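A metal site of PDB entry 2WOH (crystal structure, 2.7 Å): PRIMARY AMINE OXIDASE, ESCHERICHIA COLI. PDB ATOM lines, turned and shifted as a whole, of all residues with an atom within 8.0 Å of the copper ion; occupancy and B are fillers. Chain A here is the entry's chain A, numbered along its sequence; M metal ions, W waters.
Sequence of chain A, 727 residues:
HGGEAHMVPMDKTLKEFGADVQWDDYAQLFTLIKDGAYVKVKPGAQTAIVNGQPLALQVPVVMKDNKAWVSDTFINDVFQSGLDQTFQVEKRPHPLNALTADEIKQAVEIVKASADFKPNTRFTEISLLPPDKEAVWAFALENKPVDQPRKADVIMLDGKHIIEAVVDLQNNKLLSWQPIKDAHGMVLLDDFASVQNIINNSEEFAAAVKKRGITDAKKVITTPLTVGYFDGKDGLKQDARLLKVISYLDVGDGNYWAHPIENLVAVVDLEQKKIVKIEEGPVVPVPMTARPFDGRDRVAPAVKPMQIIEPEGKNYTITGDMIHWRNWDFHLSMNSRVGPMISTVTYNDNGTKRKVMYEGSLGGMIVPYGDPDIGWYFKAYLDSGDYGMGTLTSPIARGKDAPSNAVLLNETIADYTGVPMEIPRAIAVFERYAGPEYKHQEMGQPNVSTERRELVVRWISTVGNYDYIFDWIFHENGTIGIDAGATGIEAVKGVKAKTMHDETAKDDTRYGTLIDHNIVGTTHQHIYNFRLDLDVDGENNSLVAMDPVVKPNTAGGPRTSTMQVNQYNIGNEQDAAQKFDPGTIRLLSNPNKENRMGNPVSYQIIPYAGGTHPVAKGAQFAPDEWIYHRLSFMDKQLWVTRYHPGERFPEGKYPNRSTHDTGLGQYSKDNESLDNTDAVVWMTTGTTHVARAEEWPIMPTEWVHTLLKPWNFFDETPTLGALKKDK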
ATOM      1  N   VAL A 367      34.142 -20.467 -20.485  1.00  0.00           N
ATOM      2  CA  VAL A 367      33.767 -20.662 -21.864  1.00  0.00           C
ATOM      3  C   VAL A 367      34.213 -19.473 -22.699  1.00  0.00           C
ATOM      4  O   VAL A 367      33.440 -18.531 -22.921  1.00  0.00           O
ATOM      5  CB  VAL A 367      32.248 -20.846 -22.006  1.00  0.00           C
ATOM      6  CG1 VAL A 367      31.868 -21.082 -23.458  1.00  0.00           C
ATOM      7  CG2 VAL A 367      31.788 -22.009 -21.137  1.00  0.00           C
ATOM      8  N   TYR A 369      35.811 -17.452 -26.096  1.00  0.00           N
ATOM      9  CA  TYR A 369      35.547 -17.422 -27.528  1.00  0.00           C
ATOM     10  C   TYR A 369      36.762 -16.978 -28.341  1.00  0.00           C
ATOM     11  O   TYR A 369      37.688 -16.367 -27.801  1.00  0.00           O
ATOM     12  CB  TYR A 369      34.341 -16.523 -27.820  1.00  0.00           C
ATOM     13  CG  TYR A 369      33.028 -17.190 -27.457  1.00  0.00           C
ATOM     14  CD1 TYR A 369      32.619 -17.300 -26.136  1.00  0.00           C
ATOM     15  CD2 TYR A 369      32.212 -17.728 -28.437  1.00  0.00           C
ATOM     16  CE1 TYR A 369      31.438 -17.920 -25.807  1.00  0.00           C
ATOM     17  CE2 TYR A 369      31.021 -18.340 -28.114  1.00  0.00           C
ATOM     18  CZ  TYR A 369      30.644 -18.438 -26.803  1.00  0.00           C
ATOM     19  OH  TYR A 369      29.452 -19.050 -26.479  1.00  0.00           O
ATOM     20  N   ASN A 465      22.700 -18.539 -21.919  1.00  0.00           N
ATOM     21  CA  ASN A 465      22.294 -19.424 -23.004  1.00  0.00           C
ATOM     22  C   ASN A 465      22.803 -20.850 -22.821  1.00  0.00           C
ATOM     23  O   ASN A 465      22.213 -21.802 -23.335  1.00  0.00           O
ATOM     24  CB  ASN A 465      22.784 -18.873 -24.341  1.00  0.00           C
ATOM     25  CG  ASN A 465      24.275 -18.659 -24.357  1.00  0.00           C
ATOM     26  OD1 ASN A 465      24.844 -18.065 -23.438  1.00  0.00           O
ATOM     27  ND2 ASN A 465      24.940 -19.155 -25.399  1.00  0.00           N
ATOM     28  N   TPQ A 466      24.054 -21.180 -21.805  1.00  0.00           N
ATOM     29  CA  TPQ A 466      24.152 -22.623 -21.763  1.00  0.00           C
ATOM     30  CB  TPQ A 466      25.623 -23.052 -21.812  1.00  0.00           C
ATOM     31  C   TPQ A 466      23.525 -23.128 -20.502  1.00  0.00           C
ATOM     32  O   TPQ A 466      23.304 -22.324 -19.569  1.00  0.00           O
ATOM     33  C1  TPQ A 466      26.454 -21.926 -22.370  1.00  0.00           C
ATOM     34  C2  TPQ A 466      26.982 -21.988 -23.757  1.00  0.00           C
ATOM     35  O2  TPQ A 466      26.704 -23.067 -24.551  1.00  0.00           O
ATOM     36  C3  TPQ A 466      27.748 -20.945 -24.261  1.00  0.00           C
ATOM     37  C4  TPQ A 466      28.034 -19.847 -23.455  1.00  0.00           C
ATOM     38  O4  TPQ A 466      28.786 -18.830 -23.948  1.00  0.00           O
ATOM     39  C5  TPQ A 466      27.511 -19.787 -22.059  1.00  0.00           C
ATOM     40  O5  TPQ A 466      27.782 -18.716 -21.264  1.00  0.00           O
ATOM     41  C6  TPQ A 466      26.741 -20.827 -21.564  1.00  0.00           C
ATOM     42  N   TYR A 468      24.348 -26.663 -18.389  1.00  0.00           N
ATOM     43  CA  TYR A 468      25.355 -27.678 -18.128  1.00  0.00           C
ATOM     44  C   TYR A 468      24.836 -28.736 -17.167  1.00  0.00           C
ATOM     45  O   TYR A 468      24.152 -28.432 -16.181  1.00  0.00           O
ATOM     46  CB  TYR A 468      26.621 -27.046 -17.571  1.00  0.00           C
ATOM     47  CG  TYR A 468      27.250 -26.018 -18.497  1.00  0.00           C
ATOM     48  CD1 TYR A 468      27.800 -26.406 -19.710  1.00  0.00           C
ATOM     49  CD2 TYR A 468      27.287 -24.676 -18.153  1.00  0.00           C
ATOM     50  CE1 TYR A 468      28.376 -25.481 -20.558  1.00  0.00           C
ATOM     51  CE2 TYR A 468      27.856 -23.732 -18.994  1.00  0.00           C
ATOM     52  CZ  TYR A 468      28.404 -24.144 -20.200  1.00  0.00           C
ATOM     53  OH  TYR A 468      28.974 -23.213 -21.045  1.00  0.00           O
ATOM     54  N   ALA A 486      26.757 -30.586 -22.032  1.00  0.00           N
ATOM     55  CA  ALA A 486      26.476 -29.217 -22.445  1.00  0.00           C
ATOM     56  C   ALA A 486      25.365 -29.185 -23.486  1.00  0.00           C
ATOM     57  O   ALA A 486      25.398 -29.890 -24.485  1.00  0.00           O
ATOM     58  CB  ALA A 486      27.726 -28.560 -22.994  1.00  0.00           C
ATOM     59  N   THR A 487      24.372 -28.342 -23.227  1.00  0.00           N
ATOM     60  CA  THR A 487      23.275 -28.158 -24.164  1.00  0.00           C
ATOM     61  C   THR A 487      22.770 -26.729 -24.037  1.00  0.00           C
ATOM     62  O   THR A 487      23.419 -25.887 -23.418  1.00  0.00           O
ATOM     63  CB  THR A 487      22.137 -29.156 -23.892  1.00  0.00           C
ATOM     64  OG1 THR A 487      21.108 -29.004 -24.886  1.00  0.00           O
ATOM     65  CG2 THR A 487      21.554 -28.951 -22.506  1.00  0.00           C
ATOM     66  N   ILE A 489      21.446 -23.103 -25.897  1.00  0.00           N
ATOM     67  CA  ILE A 489      21.423 -22.261 -27.087  1.00  0.00           C
ATOM     68  C   ILE A 489      22.761 -21.614 -27.332  1.00  0.00           C
ATOM     69  O   ILE A 489      23.317 -20.964 -26.439  1.00  0.00           O
ATOM     70  CB  ILE A 489      20.381 -21.138 -26.912  1.00  0.00           C
ATOM     71  CG1 ILE A 489      19.055 -21.704 -26.400  1.00  0.00           C
ATOM     72  CG2 ILE A 489      20.191 -20.395 -28.219  1.00  0.00           C
ATOM     73  CD1 ILE A 489      18.311 -22.527 -27.418  1.00  0.00           C
ATOM     74  N   GLU A 490      23.289 -21.772 -28.541  1.00  0.00           N
ATOM     75  CA  GLU A 490      24.571 -21.168 -28.893  1.00  0.00           C
ATOM     76  C   GLU A 490      24.499 -19.650 -28.996  1.00  0.00           C
ATOM     77  O   GLU A 490      23.470 -19.084 -29.369  1.00  0.00           O
ATOM     78  CB  GLU A 490      25.091 -21.735 -30.221  1.00  0.00           C
ATOM     79  CG  GLU A 490      26.049 -22.885 -30.046  1.00  0.00           C
ATOM     80  CD  GLU A 490      26.320 -23.625 -31.340  1.00  0.00           C
ATOM     81  OE1 GLU A 490      27.051 -23.082 -32.193  1.00  0.00           O
ATOM     82  OE2 GLU A 490      25.789 -24.749 -31.495  1.00  0.00           O
ATOM     83  N   ALA A 491      25.602 -19.005 -28.656  1.00  0.00           N
ATOM     84  CA  ALA A 491      25.772 -17.581 -28.870  1.00  0.00           C
ATOM     85  C   ALA A 491      26.214 -17.395 -30.310  1.00  0.00           C
ATOM     86  O   ALA A 491      27.234 -17.934 -30.725  1.00  0.00           O
ATOM     87  CB  ALA A 491      26.826 -17.026 -27.919  1.00  0.00           C
ATOM     88  N   THR A 522      29.900 -18.797 -33.442  1.00  0.00           N
ATOM     89  CA  THR A 522      31.307 -18.488 -33.159  1.00  0.00           C
ATOM     90  C   THR A 522      31.982 -19.631 -32.420  1.00  0.00           C
ATOM     91  O   THR A 522      31.433 -20.188 -31.458  1.00  0.00           O
ATOM     92  CB  THR A 522      31.450 -17.214 -32.310  1.00  0.00           C
ATOM     93  OG1 THR A 522      30.818 -16.121 -32.978  1.00  0.00           O
ATOM     94  CG2 THR A 522      32.917 -16.896 -32.105  1.00  0.00           C
ATOM     95  N   THR A 523      33.187 -19.987 -32.872  1.00  0.00           N
ATOM     96  CA  THR A 523      33.949 -21.073 -32.280  1.00  0.00           C
ATOM     97  C   THR A 523      34.376 -20.711 -30.853  1.00  0.00           C
ATOM     98  O   THR A 523      34.728 -19.564 -30.574  1.00  0.00           O
ATOM     99  CB  THR A 523      35.200 -21.415 -33.125  1.00  0.00           C
ATOM    100  OG1 THR A 523      34.784 -21.957 -34.385  1.00  0.00           O
ATOM    101  CG2 THR A 523      36.078 -22.426 -32.420  1.00  0.00           C
ATOM    102  N   HIS A 524      34.324 -21.689 -29.960  1.00  0.00           N
ATOM    103  CA  HIS A 524      34.720 -21.472 -28.574  1.00  0.00           C
ATOM    104  C   HIS A 524      35.164 -22.779 -27.951  1.00  0.00           C
ATOM    105  O   HIS A 524      35.189 -23.821 -28.599  1.00  0.00           O
ATOM    106  CB  HIS A 524      33.543 -20.901 -27.777  1.00  0.00           C
ATOM    107  CG  HIS A 524      32.306 -21.734 -27.869  1.00  0.00           C
ATOM    108  ND1 HIS A 524      31.581 -21.856 -29.029  1.00  0.00           N
ATOM    109  CD2 HIS A 524      31.672 -22.508 -26.942  1.00  0.00           C
ATOM    110  CE1 HIS A 524      30.538 -22.655 -28.820  1.00  0.00           C
ATOM    111  NE2 HIS A 524      30.575 -23.060 -27.563  1.00  0.00           N
ATOM    112  N   GLN A 525      35.529 -22.713 -26.673  1.00  0.00           N
ATOM    113  CA  GLN A 525      35.847 -23.897 -25.904  1.00  0.00           C
ATOM    114  C   GLN A 525      34.964 -23.970 -24.663  1.00  0.00           C
ATOM    115  O   GLN A 525      34.545 -22.942 -24.129  1.00  0.00           O
ATOM    116  CB  GLN A 525      37.299 -23.869 -25.447  1.00  0.00           C
ATOM    117  CG  GLN A 525      38.308 -23.905 -26.566  1.00  0.00           C
ATOM    118  CD  GLN A 525      39.715 -23.987 -26.036  1.00  0.00           C
ATOM    119  OE1 GLN A 525      40.294 -22.985 -25.607  1.00  0.00           O
ATOM    120  NE2 GLN A 525      40.267 -25.200 -26.047  1.00  0.00           N
ATOM    121  N   HIS A 526      34.696 -25.195 -24.220  1.00  0.00           N
ATOM    122  CA  HIS A 526      34.118 -25.417 -22.907  1.00  0.00           C
ATOM    123  C   HIS A 526      35.206 -26.069 -22.058  1.00  0.00           C
ATOM    124  O   HIS A 526      35.721 -27.126 -22.417  1.00  0.00           O
ATOM    125  CB  HIS A 526      32.919 -26.356 -23.006  1.00  0.00           C
ATOM    126  CG  HIS A 526      31.787 -25.805 -23.815  1.00  0.00           C
ATOM    127  ND1 HIS A 526      30.846 -24.950 -23.297  1.00  0.00           N
ATOM    128  CD2 HIS A 526      31.440 -26.012 -25.108  1.00  0.00           C
ATOM    129  CE1 HIS A 526      29.967 -24.642 -24.232  1.00  0.00           C
ATOM    130  NE2 HIS A 526      30.305 -25.276 -25.344  1.00  0.00           N
ATOM    131  N   TYR A 528      36.025 -27.349 -18.233  1.00  0.00           N
ATOM    132  CA  TYR A 528      35.605 -27.636 -16.879  1.00  0.00           C
ATOM    133  C   TYR A 528      36.807 -28.063 -16.051  1.00  0.00           C
ATOM    134  O   TYR A 528      37.718 -28.728 -16.546  1.00  0.00           O
ATOM    135  CB  TYR A 528      34.575 -28.768 -16.859  1.00  0.00           C
ATOM    136  CG  TYR A 528      33.513 -28.687 -17.932  1.00  0.00           C
ATOM    137  CD1 TYR A 528      32.356 -27.954 -17.749  1.00  0.00           C
ATOM    138  CD2 TYR A 528      33.665 -29.378 -19.133  1.00  0.00           C
ATOM    139  CE1 TYR A 528      31.375 -27.900 -18.720  1.00  0.00           C
ATOM    140  CE2 TYR A 528      32.695 -29.319 -20.117  1.00  0.00           C
ATOM    141  CZ  TYR A 528      31.548 -28.579 -19.904  1.00  0.00           C
ATOM    142  OH  TYR A 528      30.581 -28.522 -20.879  1.00  0.00           O
ATOM    143  N   HIS A 613      32.258 -34.041 -28.359  1.00  0.00           N
ATOM    144  CA  HIS A 613      32.775 -32.925 -29.141  1.00  0.00           C
ATOM    145  C   HIS A 613      34.289 -33.042 -29.261  1.00  0.00           C
ATOM    146  O   HIS A 613      34.921 -33.758 -28.489  1.00  0.00           O
ATOM    147  CB  HIS A 613      32.441 -31.586 -28.486  1.00  0.00           C
ATOM    148  CG  HIS A 613      31.282 -30.870 -29.114  1.00  0.00           C
ATOM    149  ND1 HIS A 613      30.682 -29.775 -28.522  1.00  0.00           N
ATOM    150  CD2 HIS A 613      30.603 -31.101 -30.262  1.00  0.00           C
ATOM    151  CE1 HIS A 613      29.692 -29.354 -29.297  1.00  0.00           C
ATOM    152  NE2 HIS A 613      29.621 -30.149 -30.349  1.00  0.00           N
ATOM    153  N   THR A 687      36.198 -29.181 -24.207  1.00  0.00           N
ATOM    154  CA  THR A 687      35.906 -29.415 -25.608  1.00  0.00           C
ATOM    155  C   THR A 687      36.240 -28.163 -26.405  1.00  0.00           C
ATOM    156  O   THR A 687      36.242 -27.053 -25.875  1.00  0.00           O
ATOM    157  CB  THR A 687      34.401 -29.718 -25.826  1.00  0.00           C
ATOM    158  OG1 THR A 687      33.612 -28.597 -25.393  1.00  0.00           O
ATOM    159  CG2 THR A 687      33.988 -30.964 -25.050  1.00  0.00           C
ATOM    160  N   THR A 688      36.538 -28.355 -27.690  1.00  0.00           N
ATOM    161  CA  THR A 688      36.641 -27.244 -28.630  1.00  0.00           C
ATOM    162  C   THR A 688      35.463 -27.340 -29.583  1.00  0.00           C
ATOM    163  O   THR A 688      35.374 -28.273 -30.381  1.00  0.00           O
ATOM    164  CB  THR A 688      37.957 -27.289 -29.416  1.00  0.00           C
ATOM    165  OG1 THR A 688      39.023 -26.878 -28.558  1.00  0.00           O
ATOM    166  CG2 THR A 688      37.880 -26.369 -30.610  1.00  0.00           C
ATOM    167  N   HIS A 689      34.553 -26.387 -29.479  1.00  0.00           N
ATOM    168  CA  HIS A 689      33.268 -26.485 -30.132  1.00  0.00           C
ATOM    169  C   HIS A 689      33.251 -25.738 -31.467  1.00  0.00           C
ATOM    170  O   HIS A 689      33.271 -24.509 -31.495  1.00  0.00           O
ATOM    171  CB  HIS A 689      32.171 -25.973 -29.193  1.00  0.00           C
ATOM    172  CG  HIS A 689      30.783 -26.120 -29.736  1.00  0.00           C
ATOM    173  ND1 HIS A 689      29.680 -25.584 -29.099  1.00  0.00           N
ATOM    174  CD2 HIS A 689      30.318 -26.713 -30.865  1.00  0.00           C
ATOM    175  CE1 HIS A 689      28.594 -25.851 -29.807  1.00  0.00           C
ATOM    176  NE2 HIS A 689      28.952 -26.546 -30.874  1.00  0.00           N
ATOM    177  N   VAL A 690      33.216 -26.501 -32.549  1.00  0.00           N
ATOM    178  CA  VAL A 690      32.996 -25.939 -33.872  1.00  0.00           C
ATOM    179  C   VAL A 690      31.563 -26.251 -34.266  1.00  0.00           C
ATOM    180  O   VAL A 690      31.202 -27.400 -34.509  1.00  0.00           O
ATOM    181  CB  VAL A 690      33.964 -26.539 -34.909  1.00  0.00           C
ATOM    182  CG1 VAL A 690      33.722 -25.926 -36.267  1.00  0.00           C
ATOM    183  CG2 VAL A 690      35.400 -26.325 -34.470  1.00  0.00           C
ATOM    184  N   ALA A 691      30.753 -25.203 -34.338  1.00  0.00           N
ATOM    185  CA  ALA A 691      29.306 -25.351 -34.458  1.00  0.00           C
ATOM    186  C   ALA A 691      28.882 -26.029 -35.756  1.00  0.00           C
ATOM    187  O   ALA A 691      29.648 -26.091 -36.723  1.00  0.00           O
ATOM    188  CB  ALA A 691      28.642 -23.990 -34.335  1.00  0.00           C
ATOM    189  N   GLU A 695      22.888 -28.302 -34.470  1.00  0.00           N
ATOM    190  CA  GLU A 695      22.885 -27.747 -33.119  1.00  0.00           C
ATOM    191  C   GLU A 695      22.071 -26.453 -33.036  1.00  0.00           C
ATOM    192  O   GLU A 695      22.146 -25.730 -32.046  1.00  0.00           O
ATOM    193  CB  GLU A 695      24.324 -27.482 -32.649  1.00  0.00           C
ATOM    194  CG  GLU A 695      25.269 -28.662 -32.862  1.00  0.00           C
ATOM    195  CD  GLU A 695      26.725 -28.299 -32.665  1.00  0.00           C
ATOM    196  OE1 GLU A 695      27.059 -27.093 -32.686  1.00  0.00           O
ATOM    197  OE2 GLU A 695      27.544 -29.218 -32.492  1.00  0.00           O
ATOM    198  N   MET A 699      20.918 -27.008 -28.997  1.00  0.00           N
ATOM    199  CA  MET A 699      22.018 -27.970 -29.128  1.00  0.00           C
ATOM    200  C   MET A 699      21.804 -29.281 -28.383  1.00  0.00           C
ATOM    201  O   MET A 699      21.637 -29.283 -27.162  1.00  0.00           O
ATOM    202  CB  MET A 699      23.344 -27.366 -28.647  1.00  0.00           C
ATOM    203  CG  MET A 699      24.531 -28.313 -28.844  1.00  0.00           C
ATOM    204  SD  MET A 699      26.166 -27.637 -28.444  1.00  0.00           S
ATOM    205  CE  MET A 699      26.278 -27.972 -26.683  1.00  0.00           C
ATOM    206  N   GLU A 702      26.040 -32.633 -25.488  1.00  0.00           N
ATOM    207  CA  GLU A 702      27.352 -33.204 -25.777  1.00  0.00           C
ATOM    208  C   GLU A 702      28.071 -33.490 -24.449  1.00  0.00           C
ATOM    209  O   GLU A 702      28.020 -32.678 -23.531  1.00  0.00           O
ATOM    210  CB  GLU A 702      28.190 -32.252 -26.631  1.00  0.00           C
ATOM    211  CG  GLU A 702      27.535 -31.836 -27.935  1.00  0.00           C
ATOM    212  CD  GLU A 702      27.717 -32.854 -29.043  1.00  0.00           C
ATOM    213  OE1 GLU A 702      28.300 -33.925 -28.770  1.00  0.00           O
ATOM    214  OE2 GLU A 702      27.283 -32.589 -30.174  1.00  0.00           O
HETATM  215 CU    CU M   1      29.777 -24.927 -27.104  1.00  0.00          CU
HETATM  216  O   HOH W   1      27.705 -23.282 -26.890  1.00  0.00           O
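O of His 526 is in hydrogen-bond range of N of Thr 687 (2.8 Å). The side-chain hydroxyl of Tyr 468 is in hydrogen-bond range of a ring nitrogen (ND1) of His 526, at 3.4 Å. A ring nitrogen (ND1) of His 524 is in hydrogen-bond range of the backbone carbonyl oxygen (O) of Thr 522. A ring nitrogen (NE2) of His 689 lies within hydrogen-bond range of the side-chain carboxylate of Glu 695 (2.7 Å).
The copper ion is bound by NE2 of His 526, NE2 of His 524 and ND1 of His 689. The copper ion has three donor atoms within binding distance. Slightly farther from the copper ion lies water W1 (2.7 Å).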
